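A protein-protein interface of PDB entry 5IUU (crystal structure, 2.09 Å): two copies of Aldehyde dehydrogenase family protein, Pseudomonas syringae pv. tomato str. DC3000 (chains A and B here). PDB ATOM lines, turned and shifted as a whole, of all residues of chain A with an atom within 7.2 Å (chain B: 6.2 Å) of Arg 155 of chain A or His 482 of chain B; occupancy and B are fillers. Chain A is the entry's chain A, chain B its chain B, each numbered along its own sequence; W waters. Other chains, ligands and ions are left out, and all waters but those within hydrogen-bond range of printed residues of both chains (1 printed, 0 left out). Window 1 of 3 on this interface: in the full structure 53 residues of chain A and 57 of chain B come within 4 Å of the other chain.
The side-chain carboxylate (OE1) of Glu 141 of chain A lies within hydrogen-bond range of a ring nitrogen (NE2) of His 482 of chain B (2.6 Å).
The side-chain carboxylate (OE2) of Glu 489 of chain A is in salt-bridge range of the guanidinium group (NH2) of Arg 477 of chain B.
The guanidinium group of Arg 477 of chain B is in hydrogen-bond range of the backbone carbonyl oxygen of Leu 490 of chain A (2.8 Å).
The backbone NH (N) of Arg 155 of chain A sits at hydrogen-bond distance from the side-chain carboxylate (OD2) of Asp 140 of chain A (3.0 Å).
N of Val 153 of chain A lies within hydrogen-bond range of O of Glu 141 of chain A, at 2.8 Å.
The side-chain carboxylate (OD1) of Asp 485 of chain A is in salt-bridge range of the guanidinium group (NE) of Arg 155 of chain A.
The side-chain hydroxyl (OG1) of Thr 488 of chain A lies within hydrogen-bond range of the guanidinium group (NH1) of Arg 155 of chain A, at 3.0 Å.
N of Glu 489 of chain A lies within hydrogen-bond range of O of Glu 156 of chain A (2.6 Å).
O of Arg 477 of chain B sits close to NZ of Lys 486 of chain B (3.4 Å).
Among the printed residues, merely in contact across the chains: Val 153 of chain A with Pro 466 of chain B (3.5 Å), Leu 490 of chain A with His 482 of chain B (3.7 Å) and Arg 155 of chain A with His 482 of chain B (3.98 Å).
Of the printed residues of chain B, Glu 141 of chain A touches His 482.
Arg 155 of chain A touches one residue of chain B.
Asp 485 of chain A touches none of the printed residues of chain B.
Of the printed residues of chain B, Glu 489 of chain A touches Arg 477 (2.9 Å).
Printed residues of chain B within 4 Å of Leu 490 of chain A: Arg 477 and His 482.
The nearest residue of chain B that does not touch Arg 155 of chain A is Asp 485 of chain B (5.0 Å).
The nearest residue of chain A that does not touch His 482 of chain B is Val 153 of chain A (4.04 Å).
Of the 10 printed residues of chain B, 3 touch a printed residue of chain A.
Printed residues of chain B that touch a printed residue of chain A: Pro 466, Arg 477 and His 482.
Of the 18 printed residues of chain A, 5 touch a printed residue of chain B.
Among the printed residues, Asp or Glu carboxylates within 4 Å of a Lys or Arg side-chain nitrogen of the other chain: Glu 489 of chain A with Arg 477 of chain B.
Positions printed for both chains: 484, 485 and 486.
Water W1 lies within hydrogen-bond range of NE of Arg 477 of chain B (3.0 Å), O of Pro 466 of chain B (3.2 Å) and O of Leu 490 of chain A (3.3 Å).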
ATOM      1  N   LEU A 138      28.324 -23.071 -27.712  1.00  0.00           N
ATOM      2  CA  LEU A 138      27.085 -22.602 -27.103  1.00  0.00           C
ATOM      3  C   LEU A 138      26.044 -23.710 -27.127  1.00  0.00           C
ATOM      4  O   LEU A 138      25.976 -24.491 -28.079  1.00  0.00           O
ATOM      5  CB  LEU A 138      26.544 -21.377 -27.849  1.00  0.00           C
ATOM      6  CG  LEU A 138      27.376 -20.100 -27.890  1.00  0.00           C
ATOM      7  CD1 LEU A 138      26.727 -19.081 -28.828  1.00  0.00           C
ATOM      8  CD2 LEU A 138      27.507 -19.530 -26.500  1.00  0.00           C
ATOM      9  N   TYR A 139      25.229 -23.771 -26.078  1.00  0.00           N
ATOM     10  CA  TYR A 139      24.157 -24.748 -25.972  1.00  0.00           C
ATOM     11  C   TYR A 139      22.851 -24.021 -25.690  1.00  0.00           C
ATOM     12  O   TYR A 139      22.814 -23.104 -24.870  1.00  0.00           O
ATOM     13  CB  TYR A 139      24.452 -25.775 -24.861  1.00  0.00           C
ATOM     14  CG  TYR A 139      25.584 -26.701 -25.247  1.00  0.00           C
ATOM     15  CD1 TYR A 139      26.914 -26.300 -25.114  1.00  0.00           C
ATOM     16  CD2 TYR A 139      25.327 -27.959 -25.797  1.00  0.00           C
ATOM     17  CE1 TYR A 139      27.961 -27.135 -25.496  1.00  0.00           C
ATOM     18  CE2 TYR A 139      26.361 -28.794 -26.188  1.00  0.00           C
ATOM     19  CZ  TYR A 139      27.679 -28.377 -26.031  1.00  0.00           C
ATOM     20  OH  TYR A 139      28.712 -29.206 -26.403  1.00  0.00           O
ATOM     21  N   ASP A 140      21.797 -24.418 -26.383  1.00  0.00           N
ATOM     22  CA  ASP A 140      20.447 -24.024 -26.031  1.00  0.00           C
ATOM     23  C   ASP A 140      19.920 -25.019 -24.991  1.00  0.00           C
ATOM     24  O   ASP A 140      20.686 -25.795 -24.416  1.00  0.00           O
ATOM     25  CB  ASP A 140      19.598 -23.915 -27.302  1.00  0.00           C
ATOM     26  CG  ASP A 140      20.006 -22.724 -28.167  1.00  0.00           C
ATOM     27  OD1 ASP A 140      20.532 -21.740 -27.599  1.00  0.00           O
ATOM     28  OD2 ASP A 140      19.824 -22.763 -29.401  1.00  0.00           O
ATOM     29  N   GLU A 141      18.611 -25.031 -24.750  1.00  0.00           N
ATOM     30  CA  GLU A 141      18.081 -25.625 -23.532  1.00  0.00           C
ATOM     31  C   GLU A 141      16.936 -26.591 -23.801  1.00  0.00           C
ATOM     32  O   GLU A 141      16.105 -26.377 -24.691  1.00  0.00           O
ATOM     33  CB  GLU A 141      17.614 -24.532 -22.566  1.00  0.00           C
ATOM     34  CG  GLU A 141      18.789 -23.724 -22.011  1.00  0.00           C
ATOM     35  CD  GLU A 141      18.358 -22.402 -21.406  1.00  0.00           C
ATOM     36  OE1 GLU A 141      18.066 -21.461 -22.173  1.00  0.00           O
ATOM     37  OE2 GLU A 141      18.295 -22.312 -20.163  1.00  0.00           O
ATOM     38  N   VAL A 153      14.082 -24.737 -25.847  1.00  0.00           N
ATOM     39  CA  VAL A 153      14.248 -23.289 -25.808  1.00  0.00           C
ATOM     40  C   VAL A 153      15.548 -23.000 -26.546  1.00  0.00           C
ATOM     41  O   VAL A 153      16.635 -23.323 -26.051  1.00  0.00           O
ATOM     42  CB  VAL A 153      14.274 -22.734 -24.375  1.00  0.00           C
ATOM     43  CG1 VAL A 153      14.277 -21.225 -24.411  1.00  0.00           C
ATOM     44  CG2 VAL A 153      13.057 -23.224 -23.579  1.00  0.00           C
ATOM     45  N   THR A 154      15.434 -22.433 -27.747  1.00  0.00           N
ATOM     46  CA  THR A 154      16.550 -22.265 -28.664  1.00  0.00           C
ATOM     47  C   THR A 154      16.706 -20.798 -29.043  1.00  0.00           C
ATOM     48  O   THR A 154      15.801 -19.978 -28.867  1.00  0.00           O
ATOM     49  CB  THR A 154      16.371 -23.106 -29.937  1.00  0.00           C
ATOM     50  OG1 THR A 154      15.157 -22.729 -30.601  1.00  0.00           O
ATOM     51  CG2 THR A 154      16.303 -24.590 -29.591  1.00  0.00           C
ATOM     52  N   ARG A 155      17.892 -20.474 -29.535  1.00  0.00           N
ATOM     53  CA  ARG A 155      18.196 -19.137 -30.011  1.00  0.00           C
ATOM     54  C   ARG A 155      18.414 -19.197 -31.515  1.00  0.00           C
ATOM     55  O   ARG A 155      19.024 -20.144 -32.021  1.00  0.00           O
ATOM     56  CB  ARG A 155      19.421 -18.573 -29.298  1.00  0.00           C
ATOM     57  CG  ARG A 155      19.153 -18.302 -27.841  1.00  0.00           C
ATOM     58  CD  ARG A 155      20.331 -17.655 -27.161  1.00  0.00           C
ATOM     59  NE  ARG A 155      19.960 -17.158 -25.838  1.00  0.00           N
ATOM     60  CZ  ARG A 155      19.404 -15.971 -25.614  1.00  0.00           C
ATOM     61  NH1 ARG A 155      19.138 -15.144 -26.626  1.00  0.00           N
ATOM     62  NH2 ARG A 155      19.100 -15.617 -24.373  1.00  0.00           N
ATOM     63  N   GLU A 156      17.884 -18.201 -32.218  1.00  0.00           N
ATOM     64  CA  GLU A 156      18.000 -18.032 -33.658  1.00  0.00           C
ATOM     65  C   GLU A 156      18.442 -16.613 -33.972  1.00  0.00           C
ATOM     66  O   GLU A 156      18.113 -15.690 -33.228  1.00  0.00           O
ATOM     67  CB  GLU A 156      16.657 -18.287 -34.358  1.00  0.00           C
ATOM     68  CG  GLU A 156      16.104 -19.669 -34.164  1.00  0.00           C
ATOM     69  CD  GLU A 156      14.701 -19.802 -34.710  1.00  0.00           C
ATOM     70  OE1 GLU A 156      14.209 -18.833 -35.329  1.00  0.00           O
ATOM     71  OE2 GLU A 156      14.111 -20.887 -34.551  1.00  0.00           O
ATOM     72  N   PRO A 157      19.152 -16.403 -35.079  1.00  0.00           N
ATOM     73  CA  PRO A 157      19.519 -15.033 -35.469  1.00  0.00           C
ATOM     74  C   PRO A 157      18.293 -14.163 -35.702  1.00  0.00           C
ATOM     75  O   PRO A 157      17.245 -14.631 -36.144  1.00  0.00           O
ATOM     76  CB  PRO A 157      20.316 -15.236 -36.768  1.00  0.00           C
ATOM     77  CG  PRO A 157      19.910 -16.638 -37.247  1.00  0.00           C
ATOM     78  CD  PRO A 157      19.745 -17.410 -35.978  1.00  0.00           C
ATOM     79  N   THR A 184      26.537 -15.554 -35.039  1.00  0.00           N
ATOM     80  CA  THR A 184      25.211 -16.119 -34.823  1.00  0.00           C
ATOM     81  C   THR A 184      24.426 -16.278 -36.114  1.00  0.00           C
ATOM     82  O   THR A 184      23.325 -16.839 -36.075  1.00  0.00           O
ATOM     83  CB  THR A 184      24.392 -15.272 -33.826  1.00  0.00           C
ATOM     84  OG1 THR A 184      24.410 -13.886 -34.196  1.00  0.00           O
ATOM     85  CG2 THR A 184      24.980 -15.387 -32.459  1.00  0.00           C
ATOM     86  N   PHE A 484      26.290 -12.489 -27.399  1.00  0.00           N
ATOM     87  CA  PHE A 484      25.509 -13.141 -28.444  1.00  0.00           C
ATOM     88  C   PHE A 484      24.019 -12.873 -28.296  1.00  0.00           C
ATOM     89  O   PHE A 484      23.304 -12.839 -29.303  1.00  0.00           O
ATOM     90  CB  PHE A 484      25.790 -14.645 -28.446  1.00  0.00           C
ATOM     91  CG  PHE A 484      27.167 -14.998 -28.959  1.00  0.00           C
ATOM     92  CD1 PHE A 484      28.217 -15.223 -28.092  1.00  0.00           C
ATOM     93  CD2 PHE A 484      27.407 -15.097 -30.307  1.00  0.00           C
ATOM     94  CE1 PHE A 484      29.479 -15.540 -28.573  1.00  0.00           C
ATOM     95  CE2 PHE A 484      28.658 -15.428 -30.789  1.00  0.00           C
ATOM     96  CZ  PHE A 484      29.694 -15.637 -29.932  1.00  0.00           C
ATOM     97  N   ASP A 485      23.532 -12.650 -27.066  1.00  0.00           N
ATOM     98  CA  ASP A 485      22.085 -12.581 -26.850  1.00  0.00           C
ATOM     99  C   ASP A 485      21.443 -11.424 -27.609  1.00  0.00           C
ATOM    100  O   ASP A 485      20.314 -11.561 -28.088  1.00  0.00           O
ATOM    101  CB  ASP A 485      21.760 -12.468 -25.350  1.00  0.00           C
ATOM    102  CG  ASP A 485      22.220 -13.686 -24.543  1.00  0.00           C
ATOM    103  OD1 ASP A 485      22.487 -14.760 -25.140  1.00  0.00           O
ATOM    104  OD2 ASP A 485      22.311 -13.566 -23.302  1.00  0.00           O
ATOM    105  N   LYS A 486      22.143 -10.287 -27.733  1.00  0.00           N
ATOM    106  CA  LYS A 486      21.675  -9.150 -28.534  1.00  0.00           C
ATOM    107  C   LYS A 486      21.348  -9.518 -29.972  1.00  0.00           C
ATOM    108  O   LYS A 486      20.612  -8.781 -30.642  1.00  0.00           O
ATOM    109  CB  LYS A 486      22.755  -8.060 -28.604  1.00  0.00           C
ATOM    110  CG  LYS A 486      22.796  -7.131 -27.441  1.00  0.00           C
ATOM    111  CD  LYS A 486      23.746  -5.999 -27.721  1.00  0.00           C
ATOM    112  CE  LYS A 486      25.041  -6.180 -26.973  1.00  0.00           C
ATOM    113  NZ  LYS A 486      25.988  -7.031 -27.741  1.00  0.00           N
ATOM    114  N   TYR A 487      21.933 -10.591 -30.495  1.00  0.00           N
ATOM    115  CA  TYR A 487      21.833 -10.871 -31.919  1.00  0.00           C
ATOM    116  C   TYR A 487      20.973 -12.088 -32.214  1.00  0.00           C
ATOM    117  O   TYR A 487      20.947 -12.549 -33.357  1.00  0.00           O
ATOM    118  CB  TYR A 487      23.236 -11.024 -32.517  1.00  0.00           C
ATOM    119  CG  TYR A 487      24.095  -9.810 -32.251  1.00  0.00           C
ATOM    120  CD1 TYR A 487      23.891  -8.625 -32.961  1.00  0.00           C
ATOM    121  CD2 TYR A 487      25.082  -9.829 -31.274  1.00  0.00           C
ATOM    122  CE1 TYR A 487      24.677  -7.506 -32.726  1.00  0.00           C
ATOM    123  CE2 TYR A 487      25.865  -8.705 -31.020  1.00  0.00           C
ATOM    124  CZ  TYR A 487      25.659  -7.553 -31.758  1.00  0.00           C
ATOM    125  OH  TYR A 487      26.416  -6.434 -31.514  1.00  0.00           O
ATOM    126  N   THR A 488      20.247 -12.606 -31.217  1.00  0.00           N
ATOM    127  CA  THR A 488      19.417 -13.782 -31.406  1.00  0.00           C
ATOM    128  C   THR A 488      18.046 -13.550 -30.772  1.00  0.00           C
ATOM    129  O   THR A 488      17.870 -12.653 -29.946  1.00  0.00           O
ATOM    130  CB  THR A 488      20.075 -15.055 -30.809  1.00  0.00           C
ATOM    131  OG1 THR A 488      20.278 -14.886 -29.402  1.00  0.00           O
ATOM    132  CG2 THR A 488      21.430 -15.363 -31.480  1.00  0.00           C
ATOM    133  N   GLU A 489      17.077 -14.361 -31.202  1.00  0.00           N
ATOM    134  CA  GLU A 489      15.740 -14.444 -30.625  1.00  0.00           C
ATOM    135  C   GLU A 489      15.568 -15.786 -29.931  1.00  0.00           C
ATOM    136  O   GLU A 489      16.016 -16.819 -30.444  1.00  0.00           O
ATOM    137  CB  GLU A 489      14.634 -14.341 -31.690  1.00  0.00           C
ATOM    138  CG  GLU A 489      14.366 -12.996 -32.244  1.00  0.00           C
ATOM    139  CD  GLU A 489      13.750 -12.059 -31.231  1.00  0.00           C
ATOM    140  OE1 GLU A 489      13.943 -10.853 -31.424  1.00  0.00           O
ATOM    141  OE2 GLU A 489      13.065 -12.511 -30.299  1.00  0.00           O
ATOM    142  N   LEU A 490      14.873 -15.774 -28.794  1.00  0.00           N
ATOM    143  CA  LEU A 490      14.465 -17.009 -28.132  1.00  0.00           C
ATOM    144  C   LEU A 490      13.211 -17.589 -28.777  1.00  0.00           C
ATOM    145  O   LEU A 490      12.248 -16.869 -29.042  1.00  0.00           O
ATOM    146  CB  LEU A 490      14.196 -16.756 -26.654  1.00  0.00           C
ATOM    147  CG  LEU A 490      15.437 -16.612 -25.783  1.00  0.00           C
ATOM    148  CD1 LEU A 490      15.034 -16.103 -24.397  1.00  0.00           C
ATOM    149  CD2 LEU A 490      16.169 -17.929 -25.697  1.00  0.00           C
ATOM    150  N   LYS A 491      13.217 -18.896 -29.017  1.00  0.00           N
ATOM    151  CA  LYS A 491      12.018 -19.607 -29.433  1.00  0.00           C
ATOM    152  C   LYS A 491      11.764 -20.789 -28.502  1.00  0.00           C
ATOM    153  O   LYS A 491      12.703 -21.480 -28.092  1.00  0.00           O
ATOM    154  CB  LYS A 491      12.134 -20.088 -30.879  1.00  0.00           C
ATOM    155  CG  LYS A 491      10.967 -20.954 -31.345  1.00  0.00           C
ATOM    156  CD  LYS A 491      11.229 -21.558 -32.719  1.00  0.00           C
ATOM    157  CE  LYS A 491      11.027 -20.551 -33.845  1.00  0.00           C
ATOM    158  NZ  LYS A 491      11.614 -21.081 -35.121  1.00  0.00           N
ATOM    159  N   PRO B 466       9.660 -19.976 -21.929  1.00  0.00           N
ATOM    160  CA  PRO B 466       9.555 -18.522 -22.130  1.00  0.00           C
ATOM    161  C   PRO B 466       8.549 -18.190 -23.227  1.00  0.00           C
ATOM    162  O   PRO B 466       8.445 -18.895 -24.234  1.00  0.00           O
ATOM    163  CB  PRO B 466      10.981 -18.108 -22.526  1.00  0.00           C
ATOM    164  CG  PRO B 466      11.583 -19.337 -23.103  1.00  0.00           C
ATOM    165  CD  PRO B 466      10.970 -20.503 -22.353  1.00  0.00           C
ATOM    166  N   ARG B 477      10.954 -12.078 -22.983  1.00  0.00           N
ATOM    167  CA  ARG B 477      10.153 -13.267 -22.747  1.00  0.00           C
ATOM    168  C   ARG B 477       9.624 -13.250 -21.323  1.00  0.00           C
ATOM    169  O   ARG B 477      10.330 -12.845 -20.394  1.00  0.00           O
ATOM    170  CB  ARG B 477      10.968 -14.555 -22.999  1.00  0.00           C
ATOM    171  CG  ARG B 477      11.459 -14.735 -24.449  1.00  0.00           C
ATOM    172  CD  ARG B 477      10.284 -14.762 -25.426  1.00  0.00           C
ATOM    173  NE  ARG B 477      10.685 -14.952 -26.813  1.00  0.00           N
ATOM    174  CZ  ARG B 477      10.822 -13.977 -27.712  1.00  0.00           C
ATOM    175  NH1 ARG B 477      10.593 -12.710 -27.371  1.00  0.00           N
ATOM    176  NH2 ARG B 477      11.190 -14.267 -28.953  1.00  0.00           N
ATOM    177  N   LYS B 479       7.866 -15.789 -18.299  1.00  0.00           N
ATOM    178  CA  LYS B 479       8.064 -17.154 -17.802  1.00  0.00           C
ATOM    179  C   LYS B 479       9.476 -17.677 -18.088  1.00  0.00           C
ATOM    180  O   LYS B 479      10.253 -17.026 -18.802  1.00  0.00           O
ATOM    181  CB  LYS B 479       7.009 -18.110 -18.382  1.00  0.00           C
ATOM    182  CG  LYS B 479       5.566 -17.670 -18.159  1.00  0.00           C
ATOM    183  CD  LYS B 479       4.595 -18.760 -18.569  1.00  0.00           C
ATOM    184  CE  LYS B 479       4.620 -18.979 -20.069  1.00  0.00           C
ATOM    185  NZ  LYS B 479       4.119 -20.334 -20.444  1.00  0.00           N
ATOM    186  N   SER B 480       9.814 -18.845 -17.514  1.00  0.00           N
ATOM    187  CA  SER B 480      11.128 -19.493 -17.600  1.00  0.00           C
ATOM    188  C   SER B 480      12.210 -18.689 -16.881  1.00  0.00           C
ATOM    189  O   SER B 480      11.947 -17.588 -16.383  1.00  0.00           O
ATOM    190  CB  SER B 480      11.532 -19.733 -19.050  1.00  0.00           C
ATOM    191  OG  SER B 480      12.213 -18.604 -19.598  1.00  0.00           O
ATOM    192  N   LEU B 481      13.422 -19.239 -16.786  1.00  0.00           N
ATOM    193  CA  LEU B 481      14.499 -18.478 -16.166  1.00  0.00           C
ATOM    194  C   LEU B 481      14.866 -17.244 -16.982  1.00  0.00           C
ATOM    195  O   LEU B 481      15.412 -16.286 -16.422  1.00  0.00           O
ATOM    196  CB  LEU B 481      15.730 -19.363 -15.960  1.00  0.00           C
ATOM    197  CG  LEU B 481      15.496 -20.603 -15.086  1.00  0.00           C
ATOM    198  CD1 LEU B 481      16.812 -21.355 -14.867  1.00  0.00           C
ATOM    199  CD2 LEU B 481      14.869 -20.224 -13.758  1.00  0.00           C
ATOM    200  N   HIS B 482      14.555 -17.235 -18.285  1.00  0.00           N
ATOM    201  CA  HIS B 482      14.896 -16.092 -19.129  1.00  0.00           C
ATOM    202  C   HIS B 482      14.079 -14.854 -18.787  1.00  0.00           C
ATOM    203  O   HIS B 482      14.511 -13.732 -19.087  1.00  0.00           O
ATOM    204  CB  HIS B 482      14.703 -16.449 -20.600  1.00  0.00           C
ATOM    205  CG  HIS B 482      15.631 -17.517 -21.080  1.00  0.00           C
ATOM    206  ND1 HIS B 482      16.928 -17.255 -21.473  1.00  0.00           N
ATOM    207  CD2 HIS B 482      15.455 -18.852 -21.228  1.00  0.00           C
ATOM    208  CE1 HIS B 482      17.510 -18.382 -21.844  1.00  0.00           C
ATOM    209  NE2 HIS B 482      16.638 -19.365 -21.709  1.00  0.00           N
ATOM    210  N   ALA B 483      12.894 -15.028 -18.179  1.00  0.00           N
ATOM    211  CA  ALA B 483      12.109 -13.864 -17.783  1.00  0.00           C
ATOM    212  C   ALA B 483      12.864 -13.016 -16.776  1.00  0.00           C
ATOM    213  O   ALA B 483      12.717 -11.790 -16.764  1.00  0.00           O
ATOM    214  CB  ALA B 483      10.750 -14.287 -17.210  1.00  0.00           C
ATOM    215  N   PHE B 484      13.710 -13.645 -15.955  1.00  0.00           N
ATOM    216  CA  PHE B 484      14.498 -12.883 -14.996  1.00  0.00           C
ATOM    217  C   PHE B 484      15.407 -11.871 -15.681  1.00  0.00           C
ATOM    218  O   PHE B 484      15.653 -10.796 -15.118  1.00  0.00           O
ATOM    219  CB  PHE B 484      15.306 -13.832 -14.109  1.00  0.00           C
ATOM    220  CG  PHE B 484      14.464 -14.588 -13.099  1.00  0.00           C
ATOM    221  CD1 PHE B 484      13.477 -15.466 -13.504  1.00  0.00           C
ATOM    222  CD2 PHE B 484      14.658 -14.416 -11.747  1.00  0.00           C
ATOM    223  CE1 PHE B 484      12.695 -16.151 -12.566  1.00  0.00           C
ATOM    224  CE2 PHE B 484      13.888 -15.101 -10.805  1.00  0.00           C
ATOM    225  CZ  PHE B 484      12.904 -15.964 -11.220  1.00  0.00           C
ATOM    226  N   ASP B 485      15.893 -12.175 -16.899  1.00  0.00           N
ATOM    227  CA  ASP B 485      16.889 -11.311 -17.535  1.00  0.00           C
ATOM    228  C   ASP B 485      16.365  -9.896 -17.736  1.00  0.00           C
ATOM    229  O   ASP B 485      17.127  -8.932 -17.648  1.00  0.00           O
ATOM    230  CB  ASP B 485      17.334 -11.890 -18.886  1.00  0.00           C
ATOM    231  CG  ASP B 485      18.213 -13.119 -18.730  1.00  0.00           C
ATOM    232  OD1 ASP B 485      18.618 -13.417 -17.582  1.00  0.00           O
ATOM    233  OD2 ASP B 485      18.498 -13.786 -19.748  1.00  0.00           O
ATOM    234  N   LYS B 486      15.071  -9.754 -18.027  1.00  0.00           N
ATOM    235  CA  LYS B 486      14.494  -8.436 -18.274  1.00  0.00           C
ATOM    236  C   LYS B 486      14.518  -7.544 -17.043  1.00  0.00           C
ATOM    237  O   LYS B 486      14.274  -6.342 -17.159  1.00  0.00           O
ATOM    238  CB  LYS B 486      13.042  -8.576 -18.748  1.00  0.00           C
ATOM    239  CG  LYS B 486      12.840  -9.691 -19.747  1.00  0.00           C
ATOM    240  CD  LYS B 486      11.481  -9.600 -20.409  1.00  0.00           C
ATOM    241  CE  LYS B 486      10.394  -9.730 -19.378  1.00  0.00           C
ATOM    242  NZ  LYS B 486       9.046  -9.716 -20.025  1.00  0.00           N
HETATM  243  O   HOH W   1      10.359 -17.928 -26.549  1.00  0.00           O
